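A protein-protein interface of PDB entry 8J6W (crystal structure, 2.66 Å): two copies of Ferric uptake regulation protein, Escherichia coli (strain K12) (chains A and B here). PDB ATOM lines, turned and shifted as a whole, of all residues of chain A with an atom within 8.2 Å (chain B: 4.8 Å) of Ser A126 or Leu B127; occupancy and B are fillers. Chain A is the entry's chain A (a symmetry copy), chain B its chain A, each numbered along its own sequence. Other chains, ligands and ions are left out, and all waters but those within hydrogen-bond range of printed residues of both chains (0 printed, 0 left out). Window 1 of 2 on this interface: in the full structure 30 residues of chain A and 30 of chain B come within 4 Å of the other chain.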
ATOM      1  N   HIS A  71      15.630   7.125 -24.228  1.00  0.00           N
ATOM      2  CA  HIS A  71      16.224   6.110 -23.365  1.00  0.00           C
ATOM      3  C   HIS A  71      17.739   6.264 -23.338  1.00  0.00           C
ATOM      4  O   HIS A  71      18.358   6.478 -24.382  1.00  0.00           O
ATOM      5  CB  HIS A  71      15.836   4.686 -23.797  1.00  0.00           C
ATOM      6  CG  HIS A  71      15.827   3.703 -22.659  1.00  0.00           C
ATOM      7  ND1 HIS A  71      14.696   3.433 -21.917  1.00  0.00           N
ATOM      8  CD2 HIS A  71      16.822   2.955 -22.113  1.00  0.00           C
ATOM      9  CE1 HIS A  71      14.992   2.553 -20.972  1.00  0.00           C
ATOM     10  NE2 HIS A  71      16.273   2.245 -21.074  1.00  0.00           N
ATOM     11  N   HIS A  87       6.631  -4.021 -32.259  1.00  0.00           N
ATOM     12  CA  HIS A  87       7.389  -4.379 -31.062  1.00  0.00           C
ATOM     13  C   HIS A  87       8.760  -4.926 -31.417  1.00  0.00           C
ATOM     14  O   HIS A  87       8.897  -5.817 -32.260  1.00  0.00           O
ATOM     15  CB  HIS A  87       6.675  -5.421 -30.213  1.00  0.00           C
ATOM     16  CG  HIS A  87       7.438  -5.785 -28.980  1.00  0.00           C
ATOM     17  ND1 HIS A  87       7.543  -4.938 -27.898  1.00  0.00           N
ATOM     18  CD2 HIS A  87       8.173  -6.880 -28.669  1.00  0.00           C
ATOM     19  CE1 HIS A  87       8.280  -5.511 -26.959  1.00  0.00           C
ATOM     20  NE2 HIS A  87       8.667  -6.693 -27.399  1.00  0.00           N
ATOM     21  N   HIS A  88       9.772  -4.411 -30.741  1.00  0.00           N
ATOM     22  CA  HIS A  88      11.100  -4.979 -30.834  1.00  0.00           C
ATOM     23  C   HIS A  88      11.743  -4.859 -29.465  1.00  0.00           C
ATOM     24  O   HIS A  88      11.219  -4.194 -28.571  1.00  0.00           O
ATOM     25  CB  HIS A  88      11.926  -4.278 -31.908  1.00  0.00           C
ATOM     26  CG  HIS A  88      12.048  -2.802 -31.697  1.00  0.00           C
ATOM     27  ND1 HIS A  88      11.448  -1.877 -32.524  1.00  0.00           N
ATOM     28  CD2 HIS A  88      12.670  -2.088 -30.729  1.00  0.00           C
ATOM     29  CE1 HIS A  88      11.724  -0.658 -32.094  1.00  0.00           C
ATOM     30  NE2 HIS A  88      12.462  -0.761 -31.006  1.00  0.00           N
ATOM     31  N   ASP A  89      12.875  -5.517 -29.308  1.00  0.00           N
ATOM     32  CA  ASP A  89      13.693  -5.366 -28.121  1.00  0.00           C
ATOM     33  C   ASP A  89      15.014  -4.753 -28.575  1.00  0.00           C
ATOM     34  O   ASP A  89      15.146  -4.321 -29.722  1.00  0.00           O
ATOM     35  CB  ASP A  89      13.824  -6.709 -27.405  1.00  0.00           C
ATOM     36  CG  ASP A  89      12.528  -7.122 -26.729  1.00  0.00           C
ATOM     37  OD1 ASP A  89      11.999  -6.376 -25.862  1.00  0.00           O
ATOM     38  OD2 ASP A  89      12.002  -8.173 -27.135  1.00  0.00           O
ATOM     39  N   HIS A  90      16.000  -4.699 -27.685  1.00  0.00           N
ATOM     40  CA  HIS A  90      17.168  -3.868 -27.960  1.00  0.00           C
ATOM     41  C   HIS A  90      18.464  -4.611 -27.695  1.00  0.00           C
ATOM     42  O   HIS A  90      18.661  -5.164 -26.611  1.00  0.00           O
ATOM     43  CB  HIS A  90      17.124  -2.589 -27.125  1.00  0.00           C
ATOM     44  CG  HIS A  90      15.888  -1.782 -27.343  1.00  0.00           C
ATOM     45  ND1 HIS A  90      14.796  -1.867 -26.508  1.00  0.00           N
ATOM     46  CD2 HIS A  90      15.564  -0.885 -28.301  1.00  0.00           C
ATOM     47  CE1 HIS A  90      13.854  -1.048 -26.938  1.00  0.00           C
ATOM     48  NE2 HIS A  90      14.303  -0.435 -28.014  1.00  0.00           N
ATOM     49  N   ILE A 107      10.900 -16.223 -28.614  1.00  0.00           N
ATOM     50  CA  ILE A 107      11.101 -15.651 -27.291  1.00  0.00           C
ATOM     51  C   ILE A 107       9.817 -15.007 -26.787  1.00  0.00           C
ATOM     52  O   ILE A 107       9.368 -15.293 -25.671  1.00  0.00           O
ATOM     53  CB  ILE A 107      12.270 -14.650 -27.295  1.00  0.00           C
ATOM     54  CG1 ILE A 107      13.585 -15.356 -27.608  1.00  0.00           C
ATOM     55  CG2 ILE A 107      12.365 -13.952 -25.940  1.00  0.00           C
ATOM     56  CD1 ILE A 107      14.817 -14.464 -27.419  1.00  0.00           C
ATOM     57  N   GLU A 108       9.205 -14.134 -27.589  1.00  0.00           N
ATOM     58  CA  GLU A 108       7.959 -13.493 -27.158  1.00  0.00           C
ATOM     59  C   GLU A 108       6.910 -14.533 -26.786  1.00  0.00           C
ATOM     60  O   GLU A 108       6.029 -14.263 -25.962  1.00  0.00           O
ATOM     61  CB  GLU A 108       7.395 -12.561 -28.249  1.00  0.00           C
ATOM     62  CG  GLU A 108       8.382 -11.542 -28.827  1.00  0.00           C
ATOM     63  CD  GLU A 108       8.751 -10.388 -27.886  1.00  0.00           C
ATOM     64  OE1 GLU A 108       7.882  -9.861 -27.161  1.00  0.00           O
ATOM     65  OE2 GLU A 108       9.930  -9.979 -27.894  1.00  0.00           O
ATOM     66  N   GLN A 111       8.056 -16.177 -23.347  1.00  0.00           N
ATOM     67  CA  GLN A 111       7.793 -15.194 -22.307  1.00  0.00           C
ATOM     68  C   GLN A 111       6.341 -15.258 -21.854  1.00  0.00           C
ATOM     69  O   GLN A 111       6.053 -15.221 -20.654  1.00  0.00           O
ATOM     70  CB  GLN A 111       8.147 -13.802 -22.804  1.00  0.00           C
ATOM     71  CG  GLN A 111       9.631 -13.525 -22.856  1.00  0.00           C
ATOM     72  CD  GLN A 111       9.953 -12.162 -23.476  1.00  0.00           C
ATOM     73  OE1 GLN A 111       9.067 -11.452 -23.948  1.00  0.00           O
ATOM     74  NE2 GLN A 111      11.227 -11.804 -23.486  1.00  0.00           N
ATOM     75  N   ILE A 114       6.105 -18.545 -19.826  1.00  0.00           N
ATOM     76  CA  ILE A 114       6.720 -18.537 -18.498  1.00  0.00           C
ATOM     77  C   ILE A 114       5.863 -17.751 -17.509  1.00  0.00           C
ATOM     78  O   ILE A 114       5.752 -18.120 -16.335  1.00  0.00           O
ATOM     79  CB  ILE A 114       8.154 -17.981 -18.577  1.00  0.00           C
ATOM     80  CG1 ILE A 114       9.084 -19.032 -19.175  1.00  0.00           C
ATOM     81  CG2 ILE A 114       8.659 -17.516 -17.193  1.00  0.00           C
ATOM     82  CD1 ILE A 114      10.378 -18.467 -19.703  1.00  0.00           C
ATOM     83  N   LEU A 122       1.054 -12.117 -19.195  1.00  0.00           N
ATOM     84  CA  LEU A 122       2.085 -11.153 -19.565  1.00  0.00           C
ATOM     85  C   LEU A 122       1.480  -9.923 -20.216  1.00  0.00           C
ATOM     86  O   LEU A 122       0.821 -10.035 -21.259  1.00  0.00           O
ATOM     87  CB  LEU A 122       3.078 -11.799 -20.524  1.00  0.00           C
ATOM     88  CG  LEU A 122       4.313 -10.954 -20.803  1.00  0.00           C
ATOM     89  CD1 LEU A 122       5.220 -10.898 -19.540  1.00  0.00           C
ATOM     90  CD2 LEU A 122       5.036 -11.580 -21.947  1.00  0.00           C
ATOM     91  N   ASN A 124       3.549  -6.605 -20.126  1.00  0.00           N
ATOM     92  CA  ASN A 124       4.644  -5.795 -20.624  1.00  0.00           C
ATOM     93  C   ASN A 124       5.953  -6.486 -20.282  1.00  0.00           C
ATOM     94  O   ASN A 124       5.999  -7.387 -19.435  1.00  0.00           O
ATOM     95  CB  ASN A 124       4.587  -4.380 -20.043  1.00  0.00           C
ATOM     96  CG  ASN A 124       5.564  -3.429 -20.710  1.00  0.00           C
ATOM     97  OD1 ASN A 124       5.912  -3.591 -21.875  1.00  0.00           O
ATOM     98  ND2 ASN A 124       5.990  -2.414 -19.976  1.00  0.00           N
ATOM     99  N   HIS A 125       7.016  -6.066 -20.958  1.00  0.00           N
ATOM    100  CA  HIS A 125       8.325  -6.645 -20.742  1.00  0.00           C
ATOM    101  C   HIS A 125       9.366  -5.746 -21.364  1.00  0.00           C
ATOM    102  O   HIS A 125       9.071  -4.980 -22.284  1.00  0.00           O
ATOM    103  CB  HIS A 125       8.420  -8.057 -21.325  1.00  0.00           C
ATOM    104  CG  HIS A 125       8.353  -8.111 -22.817  1.00  0.00           C
ATOM    105  ND1 HIS A 125       7.160  -8.075 -23.506  1.00  0.00           N
ATOM    106  CD2 HIS A 125       9.327  -8.204 -23.751  1.00  0.00           C
ATOM    107  CE1 HIS A 125       7.403  -8.133 -24.803  1.00  0.00           C
ATOM    108  NE2 HIS A 125       8.708  -8.209 -24.975  1.00  0.00           N
ATOM    109  N   SER A 126      10.580  -5.825 -20.840  1.00  0.00           N
ATOM    110  CA  SER A 126      11.712  -5.157 -21.458  1.00  0.00           C
ATOM    111  C   SER A 126      12.894  -6.110 -21.474  1.00  0.00           C
ATOM    112  O   SER A 126      13.194  -6.782 -20.471  1.00  0.00           O
ATOM    113  CB  SER A 126      12.064  -3.839 -20.759  1.00  0.00           C
ATOM    114  OG  SER A 126      12.717  -4.050 -19.541  1.00  0.00           O
ATOM    115  N   LEU A 127      13.543  -6.181 -22.624  1.00  0.00           N
ATOM    116  CA  LEU A 127      14.652  -7.097 -22.828  1.00  0.00           C
ATOM    117  C   LEU A 127      15.787  -6.285 -23.418  1.00  0.00           C
ATOM    118  O   LEU A 127      15.686  -5.814 -24.546  1.00  0.00           O
ATOM    119  CB  LEU A 127      14.248  -8.256 -23.739  1.00  0.00           C
ATOM    120  CG  LEU A 127      15.333  -9.179 -24.287  1.00  0.00           C
ATOM    121  CD1 LEU A 127      16.255  -9.709 -23.196  1.00  0.00           C
ATOM    122  CD2 LEU A 127      14.616 -10.304 -24.968  1.00  0.00           C
ATOM    123  N   TYR A 128      16.852  -6.105 -22.652  1.00  0.00           N
ATOM    124  CA  TYR A 128      18.008  -5.356 -23.114  1.00  0.00           C
ATOM    125  C   TYR A 128      19.190  -6.308 -23.200  1.00  0.00           C
ATOM    126  O   TYR A 128      19.484  -7.027 -22.236  1.00  0.00           O
ATOM    127  CB  TYR A 128      18.290  -4.165 -22.185  1.00  0.00           C
ATOM    128  CG  TYR A 128      17.244  -3.072 -22.323  1.00  0.00           C
ATOM    129  CD1 TYR A 128      17.373  -2.075 -23.289  1.00  0.00           C
ATOM    130  CD2 TYR A 128      16.102  -3.072 -21.530  1.00  0.00           C
ATOM    131  CE1 TYR A 128      16.410  -1.094 -23.437  1.00  0.00           C
ATOM    132  CE2 TYR A 128      15.134  -2.089 -21.670  1.00  0.00           C
ATOM    133  CZ  TYR A 128      15.296  -1.108 -22.624  1.00  0.00           C
ATOM    134  OH  TYR A 128      14.332  -0.139 -22.757  1.00  0.00           O
ATOM    135  N   LEU A 129      19.819  -6.354 -24.372  1.00  0.00           N
ATOM    136  CA  LEU A 129      21.010  -7.156 -24.582  1.00  0.00           C
ATOM    137  C   LEU A 129      22.212  -6.234 -24.686  1.00  0.00           C
ATOM    138  O   LEU A 129      22.154  -5.196 -25.356  1.00  0.00           O
ATOM    139  CB  LEU A 129      20.897  -8.019 -25.846  1.00  0.00           C
ATOM    140  CG  LEU A 129      19.795  -9.089 -25.875  1.00  0.00           C
ATOM    141  CD1 LEU A 129      19.906  -9.947 -27.118  1.00  0.00           C
ATOM    142  CD2 LEU A 129      19.816  -9.950 -24.615  1.00  0.00           C
ATOM    143  N   TYR A 130      23.299  -6.620 -24.028  1.00  0.00           N
ATOM    144  CA  TYR A 130      24.531  -5.850 -24.029  1.00  0.00           C
ATOM    145  C   TYR A 130      25.680  -6.774 -24.385  1.00  0.00           C
ATOM    146  O   TYR A 130      25.666  -7.952 -24.025  1.00  0.00           O
ATOM    147  CB  TYR A 130      24.777  -5.189 -22.659  1.00  0.00           C
ATOM    148  CG  TYR A 130      23.670  -4.249 -22.218  1.00  0.00           C
ATOM    149  CD1 TYR A 130      23.637  -2.943 -22.661  1.00  0.00           C
ATOM    150  CD2 TYR A 130      22.648  -4.681 -21.367  1.00  0.00           C
ATOM    151  CE1 TYR A 130      22.634  -2.076 -22.270  1.00  0.00           C
ATOM    152  CE2 TYR A 130      21.634  -3.818 -20.962  1.00  0.00           C
ATOM    153  CZ  TYR A 130      21.632  -2.519 -21.425  1.00  0.00           C
ATOM    154  OH  TYR A 130      20.632  -1.646 -21.051  1.00  0.00           O
ATOM    155  N   ASP B  89      16.292 -14.517 -14.503  1.00  0.00           N
ATOM    156  CA  ASP B  89      15.669 -13.264 -14.881  1.00  0.00           C
ATOM    157  C   ASP B  89      14.457 -13.087 -13.972  1.00  0.00           C
ATOM    158  O   ASP B  89      14.282 -13.829 -13.004  1.00  0.00           O
ATOM    159  CB  ASP B  89      15.351 -13.272 -16.376  1.00  0.00           C
ATOM    160  CG  ASP B  89      16.605 -13.160 -17.225  1.00  0.00           C
ATOM    161  OD1 ASP B  89      17.374 -12.171 -17.092  1.00  0.00           O
ATOM    162  OD2 ASP B  89      16.852 -14.120 -17.977  1.00  0.00           O
ATOM    163  N   HIS B  90      13.615 -12.099 -14.262  1.00  0.00           N
ATOM    164  CA  HIS B  90      12.618 -11.694 -13.275  1.00  0.00           C
ATOM    165  C   HIS B  90      11.238 -11.560 -13.891  1.00  0.00           C
ATOM    166  O   HIS B  90      11.062 -10.861 -14.891  1.00  0.00           O
ATOM    167  CB  HIS B  90      13.022 -10.377 -12.615  1.00  0.00           C
ATOM    168  CG  HIS B  90      14.362 -10.429 -11.962  1.00  0.00           C
ATOM    169  ND1 HIS B  90      15.505  -9.981 -12.589  1.00  0.00           N
ATOM    170  CD2 HIS B  90      14.748 -10.881 -10.748  1.00  0.00           C
ATOM    171  CE1 HIS B  90      16.537 -10.148 -11.783  1.00  0.00           C
ATOM    172  NE2 HIS B  90      16.099 -10.678 -10.660  1.00  0.00           N
ATOM    173  N   PHE B 102      13.353 -16.981 -12.727  1.00  0.00           N
ATOM    174  CA  PHE B 102      13.190 -17.974 -13.779  1.00  0.00           C
ATOM    175  C   PHE B 102      14.416 -17.955 -14.673  1.00  0.00           C
ATOM    176  O   PHE B 102      15.079 -16.925 -14.833  1.00  0.00           O
ATOM    177  CB  PHE B 102      11.913 -17.755 -14.626  1.00  0.00           C
ATOM    178  CG  PHE B 102      11.981 -16.583 -15.616  1.00  0.00           C
ATOM    179  CD1 PHE B 102      12.511 -16.748 -16.896  1.00  0.00           C
ATOM    180  CD2 PHE B 102      11.437 -15.346 -15.290  1.00  0.00           C
ATOM    181  CE1 PHE B 102      12.561 -15.689 -17.789  1.00  0.00           C
ATOM    182  CE2 PHE B 102      11.474 -14.286 -16.186  1.00  0.00           C
ATOM    183  CZ  PHE B 102      12.045 -14.458 -17.430  1.00  0.00           C
ATOM    184  N   ILE B 107      16.098 -19.475 -24.218  1.00  0.00           N
ATOM    185  CA  ILE B 107      16.176 -18.030 -24.380  1.00  0.00           C
ATOM    186  C   ILE B 107      17.615 -17.554 -24.239  1.00  0.00           C
ATOM    187  O   ILE B 107      18.124 -16.832 -25.103  1.00  0.00           O
ATOM    188  CB  ILE B 107      15.245 -17.313 -23.386  1.00  0.00           C
ATOM    189  CG1 ILE B 107      13.785 -17.650 -23.674  1.00  0.00           C
ATOM    190  CG2 ILE B 107      15.456 -15.803 -23.469  1.00  0.00           C
ATOM    191  CD1 ILE B 107      12.794 -16.807 -22.864  1.00  0.00           C
ATOM    192  N   GLN B 111      19.492 -15.545 -27.195  1.00  0.00           N
ATOM    193  CA  GLN B 111      20.072 -14.239 -26.917  1.00  0.00           C
ATOM    194  C   GLN B 111      21.524 -14.182 -27.374  1.00  0.00           C
ATOM    195  O   GLN B 111      21.953 -13.200 -27.987  1.00  0.00           O
ATOM    196  CB  GLN B 111      19.955 -13.922 -25.436  1.00  0.00           C
ATOM    197  CG  GLN B 111      18.564 -13.528 -24.998  1.00  0.00           C
ATOM    198  CD  GLN B 111      18.457 -13.337 -23.481  1.00  0.00           C
ATOM    199  OE1 GLN B 111      19.408 -13.580 -22.741  1.00  0.00           O
ATOM    200  NE2 GLN B 111      17.292 -12.911 -23.022  1.00  0.00           N
ATOM    201  N   HIS B 125      22.859  -8.862 -19.912  1.00  0.00           N
ATOM    202  CA  HIS B 125      21.494  -8.688 -20.362  1.00  0.00           C
ATOM    203  C   HIS B 125      20.593  -8.573 -19.155  1.00  0.00           C
ATOM    204  O   HIS B 125      20.928  -9.049 -18.068  1.00  0.00           O
ATOM    205  CB  HIS B 125      21.042  -9.844 -21.257  1.00  0.00           C
ATOM    206  CG  HIS B 125      20.920 -11.156 -20.552  1.00  0.00           C
ATOM    207  ND1 HIS B 125      22.006 -11.971 -20.312  1.00  0.00           N
ATOM    208  CD2 HIS B 125      19.845 -11.798 -20.041  1.00  0.00           C
ATOM    209  CE1 HIS B 125      21.604 -13.054 -19.672  1.00  0.00           C
ATOM    210  NE2 HIS B 125      20.301 -12.971 -19.496  1.00  0.00           N
ATOM    211  N   SER B 126      19.459  -7.915 -19.346  1.00  0.00           N
ATOM    212  CA  SER B 126      18.423  -7.890 -18.328  1.00  0.00           C
ATOM    213  C   SER B 126      17.078  -8.118 -18.993  1.00  0.00           C
ATOM    214  O   SER B 126      16.767  -7.525 -20.041  1.00  0.00           O
ATOM    215  CB  SER B 126      18.433  -6.588 -17.519  1.00  0.00           C
ATOM    216  OG  SER B 126      17.900  -5.516 -18.241  1.00  0.00           O
ATOM    217  N   LEU B 127      16.296  -9.000 -18.392  1.00  0.00           N
ATOM    218  CA  LEU B 127      15.007  -9.387 -18.938  1.00  0.00           C
ATOM    219  C   LEU B 127      14.002  -9.266 -17.811  1.00  0.00           C
ATOM    220  O   LEU B 127      14.062 -10.023 -16.847  1.00  0.00           O
ATOM    221  CB  LEU B 127      15.055 -10.803 -19.510  1.00  0.00           C
ATOM    222  CG  LEU B 127      13.747 -11.492 -19.890  1.00  0.00           C
ATOM    223  CD1 LEU B 127      12.870 -10.626 -20.789  1.00  0.00           C
ATOM    224  CD2 LEU B 127      14.132 -12.760 -20.587  1.00  0.00           C
ATOM    225  N   TYR B 128      13.094  -8.309 -17.922  1.00  0.00           N
ATOM    226  CA  TYR B 128      12.069  -8.105 -16.912  1.00  0.00           C
ATOM    227  C   TYR B 128      10.716  -8.394 -17.540  1.00  0.00           C
ATOM    228  O   TYR B 128      10.396  -7.858 -18.608  1.00  0.00           O
ATOM    229  CB  TYR B 128      12.149  -6.683 -16.335  1.00  0.00           C
ATOM    230  CG  TYR B 128      13.373  -6.491 -15.457  1.00  0.00           C
ATOM    231  CD1 TYR B 128      13.339  -6.808 -14.100  1.00  0.00           C
ATOM    232  CD2 TYR B 128      14.577  -6.048 -15.995  1.00  0.00           C
ATOM    233  CE1 TYR B 128      14.458  -6.660 -13.302  1.00  0.00           C
ATOM    234  CE2 TYR B 128      15.702  -5.894 -15.200  1.00  0.00           C
ATOM    235  CZ  TYR B 128      15.633  -6.202 -13.859  1.00  0.00           C
ATOM    236  OH  TYR B 128      16.753  -6.048 -13.079  1.00  0.00           O
ATOM    237  N   LEU B 129       9.957  -9.287 -16.909  1.00  0.00           N
ATOM    238  CA  LEU B 129       8.610  -9.607 -17.345  1.00  0.00           C
ATOM    239  C   LEU B 129       7.619  -9.006 -16.363  1.00  0.00           C
ATOM    240  O   LEU B 129       7.809  -9.090 -15.145  1.00  0.00           O
ATOM    241  CB  LEU B 129       8.394 -11.123 -17.450  1.00  0.00           C
ATOM    242  CG  LEU B 129       9.242 -11.887 -18.479  1.00  0.00           C
ATOM    243  CD1 LEU B 129       8.811 -13.337 -18.564  1.00  0.00           C
ATOM    244  CD2 LEU B 129       9.193 -11.222 -19.852  1.00  0.00           C
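The backbone carbonyl oxygen of Ser B126 lies within hydrogen-bond range of the backbone NH of Tyr A128, at 3.0 Å.
The backbone NH of Tyr B128 sits at hydrogen-bond distance from the backbone carbonyl oxygen of Ser A126.
The backbone carbonyl oxygen of His B90 is in hydrogen-bond range of the backbone NH of Leu B129, 2.8 Å away.
N of His B90 lies within hydrogen-bond range of O of Leu B127.
N of Leu A129 lies within hydrogen-bond range of O of His A90, 2.8 Å away.
The side-chain amide oxygen (OE1) of Gln A111 sits close to a ring nitrogen (NE2) of His A125 (3.4 Å).
N of His A90 lies within hydrogen-bond range of O of Leu A127.
A ring nitrogen (NE2) of His B125 sits close to the side-chain amide oxygen of Gln B111 (3.4 Å).
Among the printed residues, merely in contact across the chains: Gln A111 with Leu B127 (3.4 Å), Gln A111 with Leu B129 (3.8 Å), Ile A114 with Phe B102 (3.8 Å), Leu A122 with Leu B129 (3.8 Å), Asn A124 with Leu B129 (3.8 Å), His A125 with Tyr B128 (3.2 Å), His A125 with Leu B129 (3.6 Å), Ser A126 with Ser B126 (3.7 Å), Ser A126 with Leu B127 (3.5 Å), Leu A127 with Gln B111 (3.4 Å), Leu A127 with Ser B126 (3.5 Å), Tyr A128 with His B125 (3.2 Å), Leu A129 with Gln B111 (3.8 Å) and Leu A129 with His B125 (3.6 Å).
Of the printed residues of chain B, Leu A122 touches Leu B129 (3.8 Å).
Printed residues of chain B within 4 Å of His A125: Tyr B128 and Leu B129.
Ser A126 touches just these residues of chain B: Ser B126, Leu B127 and Tyr B128.
Of the printed residues of chain B, Leu A127 touches Gln B111 and Ser B126.
Printed residues of chain B within 4 Å of Leu A129: Gln B111 (3.8 Å) and His B125 (3.6 Å).
Tyr A130 touches none of the printed residues of chain B.
Asp B89 touches none of the printed residues of chain A.
Of the printed residues of chain A, His B125 touches Tyr A128 (3.2 Å) and Leu A129 (3.6 Å).
Printed residues of chain A within 4 Å of Ser B126: Ser A126, Leu A127 and Tyr A128.
Of the printed residues of chain A, Leu B127 touches Gln A111 and Ser A126.
The nearest residue of chain A that does not touch Leu B127 is Leu A127 (4.03 Å).
Of the 10 printed residues of chain B, 7 touch a printed residue of chain A.
Hydrophobic or aromatic side chains of chain B that line the printed part of chain A: Phe B102, His B125, Leu B127 and Leu B129.
Gln A111 touches Leu B127, and with the chains exchanged Leu A127 touches Gln B111.
His A125 touches Tyr B128, and with the chains exchanged Tyr A128 touches His B125.
His A125 touches Leu B129, and with the chains exchanged Leu A129 touches His B125.
Ser B126 touches its own counterpart, Ser A126.
Of the 16 pairs that touch across the chains among the printed residues, 13 have their exchanged pair printed and touching as well.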
